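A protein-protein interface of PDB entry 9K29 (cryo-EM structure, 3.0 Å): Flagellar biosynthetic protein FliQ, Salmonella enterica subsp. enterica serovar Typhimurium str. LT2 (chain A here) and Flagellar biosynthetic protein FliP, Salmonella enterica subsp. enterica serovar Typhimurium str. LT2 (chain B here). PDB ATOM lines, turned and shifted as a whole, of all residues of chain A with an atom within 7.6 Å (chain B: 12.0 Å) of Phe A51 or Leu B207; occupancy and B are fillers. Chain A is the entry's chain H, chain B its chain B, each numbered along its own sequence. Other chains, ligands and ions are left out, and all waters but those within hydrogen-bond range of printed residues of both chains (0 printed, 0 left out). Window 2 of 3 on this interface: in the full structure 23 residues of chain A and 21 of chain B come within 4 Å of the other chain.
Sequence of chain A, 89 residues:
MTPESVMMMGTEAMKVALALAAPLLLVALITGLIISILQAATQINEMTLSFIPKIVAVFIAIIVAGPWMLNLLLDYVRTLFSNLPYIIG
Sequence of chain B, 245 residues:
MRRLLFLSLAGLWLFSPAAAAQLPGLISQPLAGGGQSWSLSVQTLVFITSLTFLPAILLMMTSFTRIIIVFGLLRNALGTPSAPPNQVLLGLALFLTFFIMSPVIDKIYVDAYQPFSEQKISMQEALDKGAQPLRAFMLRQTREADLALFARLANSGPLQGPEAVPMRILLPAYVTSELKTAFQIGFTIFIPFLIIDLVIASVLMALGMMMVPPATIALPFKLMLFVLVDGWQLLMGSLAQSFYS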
ATOM      1  N   LEU A  24     -25.268  14.164  -5.909  1.00  0.00           N
ATOM      2  CA  LEU A  24     -24.512  14.817  -4.844  1.00  0.00           C
ATOM      3  C   LEU A  24     -23.333  13.960  -4.396  1.00  0.00           C
ATOM      4  O   LEU A  24     -22.195  14.440  -4.327  1.00  0.00           O
ATOM      5  CB  LEU A  24     -25.435  15.127  -3.665  1.00  0.00           C
ATOM      6  CG  LEU A  24     -26.077  16.518  -3.630  1.00  0.00           C
ATOM      7  CD1 LEU A  24     -26.852  16.804  -4.906  1.00  0.00           C
ATOM      8  CD2 LEU A  24     -26.980  16.656  -2.417  1.00  0.00           C
ATOM      9  N   LEU A  25     -23.588  12.684  -4.095  1.00  0.00           N
ATOM     10  CA  LEU A  25     -22.503  11.799  -3.684  1.00  0.00           C
ATOM     11  C   LEU A  25     -21.485  11.621  -4.801  1.00  0.00           C
ATOM     12  O   LEU A  25     -20.277  11.571  -4.542  1.00  0.00           O
ATOM     13  CB  LEU A  25     -23.057  10.444  -3.244  1.00  0.00           C
ATOM     14  CG  LEU A  25     -24.125  10.445  -2.150  1.00  0.00           C
ATOM     15  CD1 LEU A  25     -24.637   9.036  -1.901  1.00  0.00           C
ATOM     16  CD2 LEU A  25     -23.582  11.051  -0.870  1.00  0.00           C
ATOM     17  N   ALA A  28     -19.368  14.814  -5.051  1.00  0.00           N
ATOM     18  CA  ALA A  28     -18.514  14.906  -3.872  1.00  0.00           C
ATOM     19  C   ALA A  28     -17.343  13.937  -3.971  1.00  0.00           C
ATOM     20  O   ALA A  28     -16.192  14.307  -3.709  1.00  0.00           O
ATOM     21  CB  ALA A  28     -19.332  14.639  -2.609  1.00  0.00           C
ATOM     22  N   THR A  31     -14.831  15.225  -6.781  1.00  0.00           N
ATOM     23  CA  THR A  31     -13.984  16.347  -6.384  1.00  0.00           C
ATOM     24  C   THR A  31     -13.010  15.938  -5.285  1.00  0.00           C
ATOM     25  O   THR A  31     -11.852  16.375  -5.285  1.00  0.00           O
ATOM     26  CB  THR A  31     -14.834  17.548  -5.958  1.00  0.00           C
ATOM     27  OG1 THR A  31     -13.975  18.650  -5.636  1.00  0.00           O
ATOM     28  CG2 THR A  31     -15.698  17.225  -4.757  1.00  0.00           C
ATOM     29  N   GLY A  32     -13.443  15.080  -4.356  1.00  0.00           N
ATOM     30  CA  GLY A  32     -12.524  14.587  -3.345  1.00  0.00           C
ATOM     31  C   GLY A  32     -11.383  13.790  -3.942  1.00  0.00           C
ATOM     32  O   GLY A  32     -10.227  13.950  -3.547  1.00  0.00           O
ATOM     33  N   ILE A  35      -8.958  16.218  -5.752  1.00  0.00           N
ATOM     34  CA  ILE A  35      -8.104  16.908  -4.793  1.00  0.00           C
ATOM     35  C   ILE A  35      -7.093  15.942  -4.189  1.00  0.00           C
ATOM     36  O   ILE A  35      -5.953  16.318  -3.909  1.00  0.00           O
ATOM     37  CB  ILE A  35      -8.949  17.605  -3.711  1.00  0.00           C
ATOM     38  CG1 ILE A  35      -9.874  18.641  -4.349  1.00  0.00           C
ATOM     39  CG2 ILE A  35      -8.052  18.292  -2.698  1.00  0.00           C
ATOM     40  CD1 ILE A  35      -9.141  19.728  -5.106  1.00  0.00           C
ATOM     41  N   MET A  47      -4.834  18.249   5.532  1.00  0.00           N
ATOM     42  CA  MET A  47      -5.911  17.289   5.750  1.00  0.00           C
ATOM     43  C   MET A  47      -7.246  17.805   5.221  1.00  0.00           C
ATOM     44  O   MET A  47      -7.904  17.139   4.414  1.00  0.00           O
ATOM     45  CB  MET A  47      -6.009  16.955   7.240  1.00  0.00           C
ATOM     46  CG  MET A  47      -7.067  15.922   7.580  1.00  0.00           C
ATOM     47  SD  MET A  47      -7.107  15.557   9.344  1.00  0.00           S
ATOM     48  CE  MET A  47      -7.823  17.068   9.981  1.00  0.00           C
ATOM     49  N   THR A  48      -7.662  18.994   5.663  1.00  0.00           N
ATOM     50  CA  THR A  48      -8.972  19.537   5.323  1.00  0.00           C
ATOM     51  C   THR A  48      -8.934  20.473   4.122  1.00  0.00           C
ATOM     52  O   THR A  48      -9.783  21.367   4.014  1.00  0.00           O
ATOM     53  CB  THR A  48      -9.574  20.260   6.528  1.00  0.00           C
ATOM     54  OG1 THR A  48      -8.906  21.513   6.716  1.00  0.00           O
ATOM     55  CG2 THR A  48      -9.426  19.418   7.780  1.00  0.00           C
ATOM     56  N   LEU A  49      -7.972  20.298   3.215  1.00  0.00           N
ATOM     57  CA  LEU A  49      -7.918  21.165   2.045  1.00  0.00           C
ATOM     58  C   LEU A  49      -8.997  20.805   1.034  1.00  0.00           C
ATOM     59  O   LEU A  49      -9.403  21.653   0.232  1.00  0.00           O
ATOM     60  CB  LEU A  49      -6.535  21.093   1.398  1.00  0.00           C
ATOM     61  CG  LEU A  49      -6.185  22.249   0.462  1.00  0.00           C
ATOM     62  CD1 LEU A  49      -6.100  23.538   1.258  1.00  0.00           C
ATOM     63  CD2 LEU A  49      -4.880  21.994  -0.261  1.00  0.00           C
ATOM     64  N   SER A  50      -9.473  19.559   1.056  1.00  0.00           N
ATOM     65  CA  SER A  50     -10.483  19.114   0.105  1.00  0.00           C
ATOM     66  C   SER A  50     -11.901  19.461   0.535  1.00  0.00           C
ATOM     67  O   SER A  50     -12.824  19.334  -0.276  1.00  0.00           O
ATOM     68  CB  SER A  50     -10.380  17.602  -0.103  1.00  0.00           C
ATOM     69  OG  SER A  50     -11.143  16.903   0.864  1.00  0.00           O
ATOM     70  N   PHE A  51     -12.097  19.894   1.781  1.00  0.00           N
ATOM     71  CA  PHE A  51     -13.449  20.118   2.283  1.00  0.00           C
ATOM     72  C   PHE A  51     -14.146  21.248   1.533  1.00  0.00           C
ATOM     73  O   PHE A  51     -15.301  21.110   1.118  1.00  0.00           O
ATOM     74  CB  PHE A  51     -13.411  20.416   3.780  1.00  0.00           C
ATOM     75  CG  PHE A  51     -14.723  20.881   4.332  1.00  0.00           C
ATOM     76  CD1 PHE A  51     -15.779  19.999   4.477  1.00  0.00           C
ATOM     77  CD2 PHE A  51     -14.907  22.204   4.691  1.00  0.00           C
ATOM     78  CE1 PHE A  51     -16.989  20.427   4.980  1.00  0.00           C
ATOM     79  CE2 PHE A  51     -16.115  22.638   5.192  1.00  0.00           C
ATOM     80  CZ  PHE A  51     -17.157  21.749   5.337  1.00  0.00           C
ATOM     81  N   ILE A  52     -13.464  22.384   1.371  1.00  0.00           N
ATOM     82  CA  ILE A  52     -14.079  23.525   0.688  1.00  0.00           C
ATOM     83  C   ILE A  52     -14.426  23.210  -0.763  1.00  0.00           C
ATOM     84  O   ILE A  52     -15.535  23.563  -1.199  1.00  0.00           O
ATOM     85  CB  ILE A  52     -13.184  24.771   0.831  1.00  0.00           C
ATOM     86  CG1 ILE A  52     -13.101  25.207   2.296  1.00  0.00           C
ATOM     87  CG2 ILE A  52     -13.709  25.908  -0.030  1.00  0.00           C
ATOM     88  CD1 ILE A  52     -11.890  24.673   3.034  1.00  0.00           C
ATOM     89  N   PRO A  53     -13.547  22.595  -1.567  1.00  0.00           N
ATOM     90  CA  PRO A  53     -13.975  22.196  -2.918  1.00  0.00           C
ATOM     91  C   PRO A  53     -15.146  21.231  -2.921  1.00  0.00           C
ATOM     92  O   PRO A  53     -16.000  21.319  -3.809  1.00  0.00           O
ATOM     93  CB  PRO A  53     -12.713  21.555  -3.509  1.00  0.00           C
ATOM     94  CG  PRO A  53     -11.599  22.186  -2.768  1.00  0.00           C
ATOM     95  CD  PRO A  53     -12.106  22.355  -1.372  1.00  0.00           C
ATOM     96  N   LYS A  54     -15.217  20.314  -1.954  1.00  0.00           N
ATOM     97  CA  LYS A  54     -16.359  19.405  -1.885  1.00  0.00           C
ATOM     98  C   LYS A  54     -17.647  20.163  -1.591  1.00  0.00           C
ATOM     99  O   LYS A  54     -18.694  19.884  -2.190  1.00  0.00           O
ATOM    100  CB  LYS A  54     -16.111  18.331  -0.829  1.00  0.00           C
ATOM    101  CG  LYS A  54     -15.049  17.323  -1.220  1.00  0.00           C
ATOM    102  CD  LYS A  54     -14.692  16.419  -0.059  1.00  0.00           C
ATOM    103  CE  LYS A  54     -15.829  15.473   0.259  1.00  0.00           C
ATOM    104  NZ  LYS A  54     -15.457  14.515   1.331  1.00  0.00           N
ATOM    105  N   ILE A  55     -17.588  21.126  -0.668  1.00  0.00           N
ATOM    106  CA  ILE A  55     -18.756  21.951  -0.375  1.00  0.00           C
ATOM    107  C   ILE A  55     -19.181  22.727  -1.612  1.00  0.00           C
ATOM    108  O   ILE A  55     -20.372  22.821  -1.923  1.00  0.00           O
ATOM    109  CB  ILE A  55     -18.468  22.892   0.808  1.00  0.00           C
ATOM    110  CG1 ILE A  55     -18.219  22.086   2.078  1.00  0.00           C
ATOM    111  CG2 ILE A  55     -19.620  23.861   1.014  1.00  0.00           C
ATOM    112  CD1 ILE A  55     -19.409  21.272   2.516  1.00  0.00           C
ATOM    113  N   VAL A  56     -18.214  23.293  -2.336  1.00  0.00           N
ATOM    114  CA  VAL A  56     -18.535  24.056  -3.539  1.00  0.00           C
ATOM    115  C   VAL A  56     -19.181  23.156  -4.588  1.00  0.00           C
ATOM    116  O   VAL A  56     -20.165  23.536  -5.233  1.00  0.00           O
ATOM    117  CB  VAL A  56     -17.274  24.752  -4.082  1.00  0.00           C
ATOM    118  CG1 VAL A  56     -17.500  25.241  -5.504  1.00  0.00           C
ATOM    119  CG2 VAL A  56     -16.876  25.904  -3.175  1.00  0.00           C
ATOM    120  N   ALA A  57     -18.637  21.951  -4.774  1.00  0.00           N
ATOM    121  CA  ALA A  57     -19.186  21.032  -5.763  1.00  0.00           C
ATOM    122  C   ALA A  57     -20.603  20.606  -5.401  1.00  0.00           C
ATOM    123  O   ALA A  57     -21.482  20.548  -6.268  1.00  0.00           O
ATOM    124  CB  ALA A  57     -18.278  19.811  -5.907  1.00  0.00           C
ATOM    125  N   VAL A  58     -20.846  20.303  -4.124  1.00  0.00           N
ATOM    126  CA  VAL A  58     -22.189  19.916  -3.701  1.00  0.00           C
ATOM    127  C   VAL A  58     -23.151  21.088  -3.846  1.00  0.00           C
ATOM    128  O   VAL A  58     -24.309  20.914  -4.245  1.00  0.00           O
ATOM    129  CB  VAL A  58     -22.155  19.370  -2.262  1.00  0.00           C
ATOM    130  CG1 VAL A  58     -23.547  19.367  -1.652  1.00  0.00           C
ATOM    131  CG2 VAL A  58     -21.567  17.971  -2.248  1.00  0.00           C
ATOM    132  N   PHE A  59     -22.684  22.300  -3.543  1.00  0.00           N
ATOM    133  CA  PHE A  59     -23.499  23.495  -3.727  1.00  0.00           C
ATOM    134  C   PHE A  59     -23.903  23.661  -5.185  1.00  0.00           C
ATOM    135  O   PHE A  59     -25.072  23.920  -5.495  1.00  0.00           O
ATOM    136  CB  PHE A  59     -22.717  24.715  -3.241  1.00  0.00           C
ATOM    137  CG  PHE A  59     -23.574  25.832  -2.735  1.00  0.00           C
ATOM    138  CD1 PHE A  59     -24.217  25.732  -1.514  1.00  0.00           C
ATOM    139  CD2 PHE A  59     -23.720  26.996  -3.471  1.00  0.00           C
ATOM    140  CE1 PHE A  59     -25.001  26.765  -1.043  1.00  0.00           C
ATOM    141  CE2 PHE A  59     -24.502  28.031  -3.006  1.00  0.00           C
ATOM    142  CZ  PHE A  59     -25.140  27.917  -1.791  1.00  0.00           C
ATOM    143  N   ILE A  62     -26.462  21.003  -6.187  1.00  0.00           N
ATOM    144  CA  ILE A  62     -27.794  21.310  -5.676  1.00  0.00           C
ATOM    145  C   ILE A  62     -28.426  22.444  -6.474  1.00  0.00           C
ATOM    146  O   ILE A  62     -29.620  22.406  -6.795  1.00  0.00           O
ATOM    147  CB  ILE A  62     -27.731  21.635  -4.172  1.00  0.00           C
ATOM    148  CG1 ILE A  62     -27.360  20.384  -3.374  1.00  0.00           C
ATOM    149  CG2 ILE A  62     -29.057  22.194  -3.685  1.00  0.00           C
ATOM    150  CD1 ILE A  62     -27.076  20.655  -1.916  1.00  0.00           C
ATOM    151  N   LEU B 198     -32.222   9.438   5.135  1.00  0.00           N
ATOM    152  CA  LEU B 198     -31.086   8.660   4.656  1.00  0.00           C
ATOM    153  C   LEU B 198     -30.258   9.454   3.654  1.00  0.00           C
ATOM    154  O   LEU B 198     -29.023   9.438   3.704  1.00  0.00           O
ATOM    155  CB  LEU B 198     -31.572   7.349   4.038  1.00  0.00           C
ATOM    156  CG  LEU B 198     -31.968   6.254   5.030  1.00  0.00           C
ATOM    157  CD1 LEU B 198     -32.438   5.009   4.296  1.00  0.00           C
ATOM    158  CD2 LEU B 198     -30.812   5.931   5.960  1.00  0.00           C
ATOM    159  N   VAL B 199     -30.922  10.159   2.736  1.00  0.00           N
ATOM    160  CA  VAL B 199     -30.198  10.947   1.744  1.00  0.00           C
ATOM    161  C   VAL B 199     -29.397  12.052   2.417  1.00  0.00           C
ATOM    162  O   VAL B 199     -28.225  12.276   2.087  1.00  0.00           O
ATOM    163  CB  VAL B 199     -31.171  11.509   0.692  1.00  0.00           C
ATOM    164  CG1 VAL B 199     -30.484  12.565  -0.156  1.00  0.00           C
ATOM    165  CG2 VAL B 199     -31.698  10.390  -0.188  1.00  0.00           C
ATOM    166  N   ILE B 200     -30.004  12.757   3.373  1.00  0.00           N
ATOM    167  CA  ILE B 200     -29.298  13.847   4.038  1.00  0.00           C
ATOM    168  C   ILE B 200     -28.126  13.310   4.852  1.00  0.00           C
ATOM    169  O   ILE B 200     -27.034  13.893   4.849  1.00  0.00           O
ATOM    170  CB  ILE B 200     -30.276  14.667   4.897  1.00  0.00           C
ATOM    171  CG1 ILE B 200     -31.069  15.619   4.002  1.00  0.00           C
ATOM    172  CG2 ILE B 200     -29.535  15.439   5.976  1.00  0.00           C
ATOM    173  CD1 ILE B 200     -32.133  16.394   4.722  1.00  0.00           C
ATOM    174  N   ALA B 201     -28.323  12.190   5.552  1.00  0.00           N
ATOM    175  CA  ALA B 201     -27.230  11.601   6.318  1.00  0.00           C
ATOM    176  C   ALA B 201     -26.087  11.169   5.410  1.00  0.00           C
ATOM    177  O   ALA B 201     -24.914  11.398   5.726  1.00  0.00           O
ATOM    178  CB  ALA B 201     -27.742  10.419   7.139  1.00  0.00           C
ATOM    179  N   SER B 202     -26.409  10.544   4.274  1.00  0.00           N
ATOM    180  CA  SER B 202     -25.368  10.114   3.347  1.00  0.00           C
ATOM    181  C   SER B 202     -24.617  11.305   2.768  1.00  0.00           C
ATOM    182  O   SER B 202     -23.389  11.264   2.628  1.00  0.00           O
ATOM    183  CB  SER B 202     -25.980   9.270   2.229  1.00  0.00           C
ATOM    184  OG  SER B 202     -26.831  10.052   1.412  1.00  0.00           O
ATOM    185  N   VAL B 203     -25.334  12.377   2.423  1.00  0.00           N
ATOM    186  CA  VAL B 203     -24.678  13.566   1.887  1.00  0.00           C
ATOM    187  C   VAL B 203     -23.758  14.182   2.932  1.00  0.00           C
ATOM    188  O   VAL B 203     -22.624  14.578   2.629  1.00  0.00           O
ATOM    189  CB  VAL B 203     -25.727  14.576   1.385  1.00  0.00           C
ATOM    190  CG1 VAL B 203     -25.083  15.926   1.124  1.00  0.00           C
ATOM    191  CG2 VAL B 203     -26.397  14.055   0.127  1.00  0.00           C
ATOM    192  N   LEU B 204     -24.224  14.266   4.181  1.00  0.00           N
ATOM    193  CA  LEU B 204     -23.382  14.810   5.240  1.00  0.00           C
ATOM    194  C   LEU B 204     -22.136  13.961   5.446  1.00  0.00           C
ATOM    195  O   LEU B 204     -21.032  14.495   5.586  1.00  0.00           O
ATOM    196  CB  LEU B 204     -24.176  14.927   6.540  1.00  0.00           C
ATOM    197  CG  LEU B 204     -25.263  16.002   6.570  1.00  0.00           C
ATOM    198  CD1 LEU B 204     -26.037  15.948   7.875  1.00  0.00           C
ATOM    199  CD2 LEU B 204     -24.657  17.379   6.361  1.00  0.00           C
ATOM    200  N   MET B 205     -22.289  12.633   5.451  1.00  0.00           N
ATOM    201  CA  MET B 205     -21.130  11.759   5.612  1.00  0.00           C
ATOM    202  C   MET B 205     -20.153  11.915   4.454  1.00  0.00           C
ATOM    203  O   MET B 205     -18.934  11.898   4.656  1.00  0.00           O
ATOM    204  CB  MET B 205     -21.575  10.303   5.743  1.00  0.00           C
ATOM    205  CG  MET B 205     -22.383   9.998   6.992  1.00  0.00           C
ATOM    206  SD  MET B 205     -21.480  10.296   8.522  1.00  0.00           S
ATOM    207  CE  MET B 205     -22.180  11.862   9.036  1.00  0.00           C
ATOM    208  N   ALA B 206     -20.671  12.058   3.233  1.00  0.00           N
ATOM    209  CA  ALA B 206     -19.798  12.299   2.089  1.00  0.00           C
ATOM    210  C   ALA B 206     -19.030  13.602   2.258  1.00  0.00           C
ATOM    211  O   ALA B 206     -17.834  13.673   1.954  1.00  0.00           O
ATOM    212  CB  ALA B 206     -20.613  12.322   0.799  1.00  0.00           C
ATOM    213  N   LEU B 207     -19.701  14.643   2.748  1.00  0.00           N
ATOM    214  CA  LEU B 207     -19.044  15.912   3.030  1.00  0.00           C
ATOM    215  C   LEU B 207     -18.191  15.873   4.290  1.00  0.00           C
ATOM    216  O   LEU B 207     -17.476  16.842   4.563  1.00  0.00           O
ATOM    217  CB  LEU B 207     -20.088  17.023   3.155  1.00  0.00           C
ATOM    218  CG  LEU B 207     -20.741  17.460   1.847  1.00  0.00           C
ATOM    219  CD1 LEU B 207     -21.774  18.545   2.095  1.00  0.00           C
ATOM    220  CD2 LEU B 207     -19.677  17.939   0.874  1.00  0.00           C
ATOM    221  N   GLY B 208     -18.245  14.786   5.055  1.00  0.00           N
ATOM    222  CA  GLY B 208     -17.591  14.730   6.346  1.00  0.00           C
ATOM    223  C   GLY B 208     -18.602  14.906   7.458  1.00  0.00           C
ATOM    224  O   GLY B 208     -19.439  14.025   7.681  1.00  0.00           O
ATOM    225  N   MET B 209     -18.506  16.031   8.166  1.00  0.00           N
ATOM    226  CA  MET B 209     -19.533  16.515   9.091  1.00  0.00           C
ATOM    227  C   MET B 209     -20.183  15.429   9.946  1.00  0.00           C
ATOM    228  O   MET B 209     -21.396  15.406  10.158  1.00  0.00           O
ATOM    229  CB  MET B 209     -20.589  17.325   8.341  1.00  0.00           C
ATOM    230  CG  MET B 209     -20.023  18.340   7.364  1.00  0.00           C
ATOM    231  SD  MET B 209     -21.306  19.445   6.749  1.00  0.00           S
ATOM    232  CE  MET B 209     -20.355  20.919   6.408  1.00  0.00           C
ATOM    233  N   MET B 210     -19.354  14.509  10.440  1.00  0.00           N
ATOM    234  CA  MET B 210     -19.858  13.511  11.375  1.00  0.00           C
ATOM    235  C   MET B 210     -20.365  14.080  12.691  1.00  0.00           C
ATOM    236  O   MET B 210     -21.003  13.349  13.456  1.00  0.00           O
ATOM    237  CB  MET B 210     -18.799  12.440  11.636  1.00  0.00           C
ATOM    238  CG  MET B 210     -18.451  11.631  10.397  1.00  0.00           C
ATOM    239  SD  MET B 210     -17.256  10.314  10.689  1.00  0.00           S
ATOM    240  CE  MET B 210     -15.745  11.251  10.867  1.00  0.00           C
ATOM    241  N   MET B 211     -20.104  15.357  12.969  1.00  0.00           N
ATOM    242  CA  MET B 211     -20.609  16.013  14.164  1.00  0.00           C
ATOM    243  C   MET B 211     -21.973  16.653  13.960  1.00  0.00           C
ATOM    244  O   MET B 211     -22.668  16.921  14.945  1.00  0.00           O
ATOM    245  CB  MET B 211     -19.627  17.096  14.631  1.00  0.00           C
ATOM    246  CG  MET B 211     -18.238  16.589  14.993  1.00  0.00           C
ATOM    247  SD  MET B 211     -18.146  15.204  16.146  1.00  0.00           S
ATOM    248  CE  MET B 211     -19.374  15.672  17.359  1.00  0.00           C
ATOM    249  N   VAL B 212     -22.364  16.903  12.715  1.00  0.00           N
ATOM    250  CA  VAL B 212     -23.627  17.566  12.407  1.00  0.00           C
ATOM    251  C   VAL B 212     -24.769  16.563  12.522  1.00  0.00           C
ATOM    252  O   VAL B 212     -24.770  15.544  11.818  1.00  0.00           O
ATOM    253  CB  VAL B 212     -23.592  18.199  11.009  1.00  0.00           C
ATOM    254  CG1 VAL B 212     -24.870  18.967  10.750  1.00  0.00           C
ATOM    255  CG2 VAL B 212     -22.387  19.111  10.880  1.00  0.00           C
ATOM    256  N   PRO B 213     -25.750  16.803  13.385  1.00  0.00           N
ATOM    257  CA  PRO B 213     -26.914  15.920  13.444  1.00  0.00           C
ATOM    258  C   PRO B 213     -27.803  16.121  12.230  1.00  0.00           C
ATOM    259  O   PRO B 213     -28.232  17.249  11.943  1.00  0.00           O
ATOM    260  CB  PRO B 213     -27.623  16.351  14.736  1.00  0.00           C
ATOM    261  CG  PRO B 213     -27.189  17.749  14.961  1.00  0.00           C
ATOM    262  CD  PRO B 213     -25.809  17.879  14.389  1.00  0.00           C
ATOM    263  N   PRO B 214     -28.097  15.052  11.488  1.00  0.00           N
ATOM    264  CA  PRO B 214     -28.906  15.207  10.268  1.00  0.00           C
ATOM    265  C   PRO B 214     -30.332  15.652  10.527  1.00  0.00           C
ATOM    266  O   PRO B 214     -30.997  16.105   9.589  1.00  0.00           O
ATOM    267  CB  PRO B 214     -28.865  13.808   9.641  1.00  0.00           C
ATOM    268  CG  PRO B 214     -28.626  12.898  10.790  1.00  0.00           C
ATOM    269  CD  PRO B 214     -27.732  13.648  11.733  1.00  0.00           C
ATOM    270  N   ILE B 217     -31.232  19.327   9.728  1.00  0.00           N
ATOM    271  CA  ILE B 217     -31.405  19.640   8.314  1.00  0.00           C
ATOM    272  C   ILE B 217     -32.640  18.951   7.748  1.00  0.00           C
ATOM    273  O   ILE B 217     -33.344  19.514   6.907  1.00  0.00           O
ATOM    274  CB  ILE B 217     -30.134  19.256   7.527  1.00  0.00           C
ATOM    275  CG1 ILE B 217     -28.932  20.071   8.006  1.00  0.00           C
ATOM    276  CG2 ILE B 217     -30.338  19.466   6.036  1.00  0.00           C
ATOM    277  CD1 ILE B 217     -28.080  19.366   9.035  1.00  0.00           C
ATOM    278  N   PHE B 221     -36.480  20.337   5.775  1.00  0.00           N
ATOM    279  CA  PHE B 221     -36.770  19.745   4.472  1.00  0.00           C
ATOM    280  C   PHE B 221     -38.019  18.877   4.523  1.00  0.00           C
ATOM    281  O   PHE B 221     -38.776  18.807   3.549  1.00  0.00           O
ATOM    282  CB  PHE B 221     -35.571  18.944   3.970  1.00  0.00           C
ATOM    283  CG  PHE B 221     -34.516  19.786   3.315  1.00  0.00           C
ATOM    284  CD1 PHE B 221     -34.821  20.560   2.208  1.00  0.00           C
ATOM    285  CD2 PHE B 221     -33.222  19.808   3.804  1.00  0.00           C
ATOM    286  CE1 PHE B 221     -33.856  21.339   1.600  1.00  0.00           C
ATOM    287  CE2 PHE B 221     -32.252  20.586   3.201  1.00  0.00           C
ATOM    288  CZ  PHE B 221     -32.569  21.351   2.097  1.00  0.00           C
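Phe A51 touches just these residues of chain B: Leu B207 (3.6 Å) and Met B209 (3.5 Å). Of chain A, only Phe A51, Lys A54, Ile A55 and Val A58 come within 4 Å of Leu B207. No residue of chain B comes within 4 Å of Ala A28. No residue of chain B comes within 4 Å of Thr A48. No residue of chain B comes within 4 Å of Leu A49. No residue of chain B comes within 4 Å of Ser A50. Ile A52 touches none of the printed residues of chain B. Of chain B, only Ala B206 (2.6 Å) and Leu B207 (3.8 Å) come within 4 Å of Lys A54. Ile A55 touches just one residue of chain B: Leu B207 (3.6 Å). Ala A57 touches none of the printed residues of chain B. Val A58 touches one residue of chain B. Ala B206 touches two residues of chain A. Printed residues of chain A within 4 Å of Val B203: Leu A24 and Leu A25. Of the printed residues of chain B, Leu A25 touches Ser B202, Val B203 and Ala B206. Of the printed residues of chain B, Leu A24 touches Val B203 (3.7 Å). Of the printed residues of chain A, Met B209 touches Phe A51 (3.5 Å). Met A47 touches none of the printed residues of chain B. Pro B213 touches none of the printed residues of chain A. The nearest residue of chain B that does not touch Phe A51 is Gly B208 (5.8 Å). The nearest residue of chain A that does not touch Leu B207 is Ala A28 (4.8 Å). The nearest printed residue of chain B that does not touch Leu A24 is Ala B206 (5.8 Å).
Hydrophobic or aromatic side chains of chain B within 4 Å of the printed part of chain A: Val B203, Ala B206, Leu B207 and Met B209. Printed residues of chain A that touch a printed residue of chain B: Leu A24, Leu A25, Phe A51, Lys A54, Ile A55 and Val A58. Along chain A the printed residues that touch a printed residue of chain B span positions 24 to 58. Among the printed residues, 10 pairs touch across the chains.
CD2 of Leu A24 touches CG2 of Val B203, at 3.7 Å. O of Ser B202 touches CD2 of Leu A25, 3.5 Å away. CD2 of Leu A25 touches CA of Val B203, 3.9 Å away. Ala B206 touches Leu A25. Leu B207 touches Phe A51. Met B209 touches Phe A51. Lys A54 touches Leu B207. Ile A55 touches Leu B207 (CD1 to CD1, 3.6 Å). Val A58 touches Leu B207 (CG2 to CD2, 3.6 Å).
NZ of Lys A54 sits at hydrogen-bond distance from O of Ala B206, at 2.6 Å.
The side-chain hydroxyl of Ser B202 lies within hydrogen-bond range of the backbone carbonyl oxygen of Val B199, 2.7 Å away. The side-chain hydroxyl (OG) of Ser B202 sits at hydrogen-bond distance from the backbone carbonyl oxygen (O) of Leu B198 (3.2 Å).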
